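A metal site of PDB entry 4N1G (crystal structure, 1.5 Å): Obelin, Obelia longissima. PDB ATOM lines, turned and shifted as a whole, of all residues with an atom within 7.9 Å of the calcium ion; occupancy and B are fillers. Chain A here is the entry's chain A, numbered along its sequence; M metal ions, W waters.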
ATOM      1  N   LYS A   4      -1.400  16.332   9.582  1.00  0.00           N
ATOM      2  CA  LYS A   4      -0.296  16.349   8.655  1.00  0.00           C
ATOM      3  C   LYS A   4      -0.233  17.587   7.747  1.00  0.00           C
ATOM      4  O   LYS A   4       0.837  17.937   7.243  1.00  0.00           O
ATOM      5  CB  LYS A   4      -0.348  15.104   7.809  1.00  0.00           C
ATOM      6  CG  LYS A   4      -1.398  15.080   6.794  1.00  0.00           C
ATOM      7  CD  LYS A   4      -1.346  13.660   6.095  1.00  0.00           C
ATOM      8  CE  LYS A   4      -2.557  13.477   5.240  1.00  0.00           C
ATOM      9  NZ  LYS A   4      -2.755  12.016   4.948  1.00  0.00           N
ATOM     10  N   THR A 129       2.696   3.819   0.126  1.00  0.00           N
ATOM     11  CA  THR A 129       2.885   4.069   1.574  1.00  0.00           C
ATOM     12  C   THR A 129       4.152   3.368   2.037  1.00  0.00           C
ATOM     13  O   THR A 129       4.646   2.414   1.406  1.00  0.00           O
ATOM     14  CB  THR A 129       1.686   3.607   2.479  1.00  0.00           C
ATOM     15  OG1 THR A 129       1.484   2.206   2.357  1.00  0.00           O
ATOM     16  CG2 THR A 129       0.390   4.338   2.141  1.00  0.00           C
ATOM     17  N   ILE A 130       4.687   3.840   3.169  1.00  0.00           N
ATOM     18  CA  ILE A 130       5.887   3.318   3.799  1.00  0.00           C
ATOM     19  C   ILE A 130       5.430   2.412   4.950  1.00  0.00           C
ATOM     20  O   ILE A 130       4.766   2.874   5.915  1.00  0.00           O
ATOM     21  CB  ILE A 130       6.851   4.470   4.316  1.00  0.00           C
ATOM     22  CG1 ILE A 130       7.143   5.471   3.198  1.00  0.00           C
ATOM     23  CG2 ILE A 130       8.138   3.908   4.931  1.00  0.00           C
ATOM     24  CD1 ILE A 130       7.621   4.821   1.906  1.00  0.00           C
ATOM     25  N   PHE A 155       8.685   5.875  13.681  1.00  0.00           N
ATOM     26  CA  PHE A 155       7.649   5.450  12.727  1.00  0.00           C
ATOM     27  C   PHE A 155       6.260   5.759  13.293  1.00  0.00           C
ATOM     28  O   PHE A 155       5.421   6.409  12.625  1.00  0.00           O
ATOM     29  CB  PHE A 155       7.771   3.942  12.423  1.00  0.00           C
ATOM     30  CG  PHE A 155       6.800   3.461  11.401  1.00  0.00           C
ATOM     31  CD1 PHE A 155       7.132   3.585  10.069  1.00  0.00           C
ATOM     32  CD2 PHE A 155       5.571   2.881  11.767  1.00  0.00           C
ATOM     33  CE1 PHE A 155       6.233   3.084   9.079  1.00  0.00           C
ATOM     34  CE2 PHE A 155       4.665   2.388  10.805  1.00  0.00           C
ATOM     35  CZ  PHE A 155       5.000   2.503   9.469  1.00  0.00           C
ATOM     36  N   ARG A 156       6.056   5.339  14.527  1.00  0.00           N
ATOM     37  CA  ARG A 156       4.766   5.546  15.199  1.00  0.00           C
ATOM     38  C   ARG A 156       4.473   7.038  15.352  1.00  0.00           C
ATOM     39  O   ARG A 156       3.352   7.463  15.064  1.00  0.00           O
ATOM     40  CB  ARG A 156       4.745   4.865  16.563  1.00  0.00           C
ATOM     41  CG  ARG A 156       4.972   3.351  16.532  1.00  0.00           C
ATOM     42  CD  ARG A 156       3.725   2.648  15.990  1.00  0.00           C
ATOM     43  NE  ARG A 156       4.051   1.223  15.879  1.00  0.00           N
ATOM     44  CZ  ARG A 156       3.792   0.458  14.818  1.00  0.00           C
ATOM     45  NH1 ARG A 156       3.153   0.970  13.771  1.00  0.00           N
ATOM     46  NH2 ARG A 156       4.191  -0.797  14.815  1.00  0.00           N
ATOM     47  N   CYS A 158       5.623   9.451  13.398  1.00  0.00           N
ATOM     48  CA  CYS A 158       5.355   9.978  12.066  1.00  0.00           C
ATOM     49  C   CYS A 158       3.927   9.646  11.601  1.00  0.00           C
ATOM     50  O   CYS A 158       3.321  10.417  10.821  1.00  0.00           O
ATOM     51  CB  CYS A 158       6.368   9.427  11.096  1.00  0.00           C
ATOM     52  SG  CYS A 158       6.263  10.183   9.469  1.00  0.00           S
ATOM     53  N   ASP A 159       3.410   8.498  12.046  1.00  0.00           N
ATOM     54  CA  ASP A 159       2.095   8.004  11.627  1.00  0.00           C
ATOM     55  C   ASP A 159       0.988   8.757  12.364  1.00  0.00           C
ATOM     56  O   ASP A 159       0.307   8.196  13.271  1.00  0.00           O
ATOM     57  CB  ASP A 159       2.026   6.513  11.884  1.00  0.00           C
ATOM     58  CG  ASP A 159       0.782   5.876  11.318  1.00  0.00           C
ATOM     59  OD1 ASP A 159       0.065   6.534  10.512  1.00  0.00           O
ATOM     60  OD2 ASP A 159       0.535   4.686  11.661  1.00  0.00           O
ATOM     61  N   LEU A 160       0.738  10.016  11.944  1.00  0.00           N
ATOM     62  CA  LEU A 160      -0.230  10.894  12.666  1.00  0.00           C
ATOM     63  C   LEU A 160      -1.664  10.342  12.707  1.00  0.00           C
ATOM     64  O   LEU A 160      -2.393  10.568  13.698  1.00  0.00           O
ATOM     65  CB  LEU A 160      -0.247  12.268  12.018  1.00  0.00           C
ATOM     66  CG  LEU A 160       1.065  13.064  12.145  1.00  0.00           C
ATOM     67  CD1 LEU A 160       1.124  14.317  11.278  1.00  0.00           C
ATOM     68  CD2 LEU A 160       1.171  13.464  13.565  1.00  0.00           C
ATOM     69  N   ASP A 161      -2.112   9.630  11.662  1.00  0.00           N
ATOM     70  CA  ASP A 161      -3.458   9.080  11.667  1.00  0.00           C
ATOM     71  C   ASP A 161      -3.538   7.599  12.125  1.00  0.00           C
ATOM     72  O   ASP A 161      -4.600   6.999  12.030  1.00  0.00           O
ATOM     73  CB  ASP A 161      -4.078   9.283  10.291  1.00  0.00           C
ATOM     74  CG  ASP A 161      -3.486   8.423   9.209  1.00  0.00           C
ATOM     75  OD1 ASP A 161      -2.509   7.701   9.444  1.00  0.00           O
ATOM     76  OD2 ASP A 161      -4.002   8.427   8.062  1.00  0.00           O
ATOM     77  N   ASN A 162      -2.406   7.077  12.671  1.00  0.00           N
ATOM     78  CA  ASN A 162      -2.308   5.716  13.198  1.00  0.00           C
ATOM     79  C   ASN A 162      -2.876   4.676  12.182  1.00  0.00           C
ATOM     80  O   ASN A 162      -3.536   3.687  12.548  1.00  0.00           O
ATOM     81  CB  ASN A 162      -2.977   5.618  14.610  1.00  0.00           C
ATOM     82  CG  ASN A 162      -2.390   6.613  15.637  1.00  0.00           C
ATOM     83  OD1 ASN A 162      -1.179   6.823  15.708  1.00  0.00           O
ATOM     84  ND2 ASN A 162      -3.271   7.235  16.429  1.00  0.00           N
ATOM     85  N   SER A 163      -2.574   4.896  10.896  1.00  0.00           N
ATOM     86  CA  SER A 163      -3.036   3.969   9.851  1.00  0.00           C
ATOM     87  C   SER A 163      -2.179   2.716   9.841  1.00  0.00           C
ATOM     88  O   SER A 163      -2.556   1.701   9.276  1.00  0.00           O
ATOM     89  CB  SER A 163      -2.964   4.639   8.462  1.00  0.00           C
ATOM     90  OG  SER A 163      -1.620   5.013   8.091  1.00  0.00           O
ATOM     91  N   GLY A 164      -1.020   2.803  10.481  1.00  0.00           N
ATOM     92  CA  GLY A 164      -0.048   1.714  10.457  1.00  0.00           C
ATOM     93  C   GLY A 164       0.959   1.800   9.322  1.00  0.00           C
ATOM     94  O   GLY A 164       1.712   0.831   9.066  1.00  0.00           O
ATOM     95  N   ASP A 165       0.908   2.885   8.556  1.00  0.00           N
ATOM     96  CA  ASP A 165       1.875   3.146   7.485  1.00  0.00           C
ATOM     97  C   ASP A 165       1.997   4.629   7.249  1.00  0.00           C
ATOM     98  O   ASP A 165       1.179   5.425   7.824  1.00  0.00           O
ATOM     99  CB  ASP A 165       1.522   2.411   6.178  1.00  0.00           C
ATOM    100  CG  ASP A 165       0.114   2.674   5.658  1.00  0.00           C
ATOM    101  OD1 ASP A 165      -0.627   3.591   6.118  1.00  0.00           O
ATOM    102  OD2 ASP A 165      -0.290   1.907   4.735  1.00  0.00           O
ATOM    103  N   LEU A 166       3.020   5.030   6.498  1.00  0.00           N
ATOM    104  CA  LEU A 166       3.296   6.467   6.318  1.00  0.00           C
ATOM    105  C   LEU A 166       2.999   6.912   4.903  1.00  0.00           C
ATOM    106  O   LEU A 166       3.350   6.218   3.908  1.00  0.00           O
ATOM    107  CB  LEU A 166       4.756   6.821   6.619  1.00  0.00           C
ATOM    108  CG  LEU A 166       5.236   6.236   7.934  1.00  0.00           C
ATOM    109  CD1 LEU A 166       6.728   6.613   8.070  1.00  0.00           C
ATOM    110  CD2 LEU A 166       4.445   6.819   9.095  1.00  0.00           C
ATOM    111  N   ASP A 167       2.334   8.050   4.760  1.00  0.00           N
ATOM    112  CA  ASP A 167       2.264   8.679   3.472  1.00  0.00           C
ATOM    113  C   ASP A 167       3.240   9.861   3.359  1.00  0.00           C
ATOM    114  O   ASP A 167       3.934  10.264   4.321  1.00  0.00           O
ATOM    115  CB  ASP A 167       0.825   9.079   3.159  1.00  0.00           C
ATOM    116  CG  ASP A 167       0.262  10.081   4.131  1.00  0.00           C
ATOM    117  OD1 ASP A 167       0.898  11.141   4.286  1.00  0.00           O
ATOM    118  OD2 ASP A 167      -0.897   9.851   4.622  1.00  0.00           O
ATOM    119  N   GLU A 170       2.737  12.771   5.682  1.00  0.00           N
ATOM    120  CA  GLU A 170       3.195  12.538   7.070  1.00  0.00           C
ATOM    121  C   GLU A 170       4.710  12.680   7.196  1.00  0.00           C
ATOM    122  O   GLU A 170       5.224  13.367   8.103  1.00  0.00           O
ATOM    123  CB  GLU A 170       2.758  11.144   7.535  1.00  0.00           C
ATOM    124  CG  GLU A 170       1.287  11.101   7.821  1.00  0.00           C
ATOM    125  CD  GLU A 170       0.771   9.710   8.059  1.00  0.00           C
ATOM    126  OE1 GLU A 170       1.314   8.733   7.456  1.00  0.00           O
ATOM    127  OE2 GLU A 170      -0.221   9.555   8.870  1.00  0.00           O
HETATM  128 CA    CA M   1      -0.487   7.100   8.301  1.00  0.00          CA
HETATM  129  O   HOH W   1      -1.377   7.628   6.240  1.00  0.00           O
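The side-chain hydroxyl (OG1) of Thr 129 sits at hydrogen-bond distance from the side-chain carboxylate (OD2) of Asp 165 (3.0 Å). The backbone NH of Gly 164 is in hydrogen-bond range of the side-chain carboxylate of Asp 159, 2.7 Å away. OD1 of Asp 167 sits at hydrogen-bond distance from N of Glu 170, 2.8 Å away. O of Asp 159 sits close to OD1 of Asn 162 (3.2 Å). N of Leu 160 sits close to OE2 of Glu 170 (3.3 Å). The backbone carbonyl oxygen (O) of Glu 170 sits at hydrogen-bond distance from the side-chain sulfur (SG) of Cys 158 (3.6 Å).
Within 4 Å of the calcium ion: Asp 159, Asp 161, Ser 163, Asp 165 and Glu 170. Along chain A the residues within 4 Å of the calcium ion span positions 159 to 170.
Water W1 is bound to the calcium ion (2.3 Å). The calcium ion is bound by OD1 of Asp 159, 2.3 Å away. The side-chain hydroxyl (OG) of Ser 163 is bound to the calcium ion (2.4 Å). The side-chain carboxylate (OD1) of Asp 161 is bound to the calcium ion (2.4 Å). The calcium ion is bound by O of Asp 165, at 2.4 Å. The calcium ion is bound by the side-chain carboxylate (OE2) of Glu 170 (2.5 Å). The calcium ion is bound by OE1 of Glu 170, 2.6 Å away.
Water W1 bridges the side-chain carboxylate of Asp 167 (2.8 Å) and the side-chain carboxylate of Asp 161 (3.3 Å).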
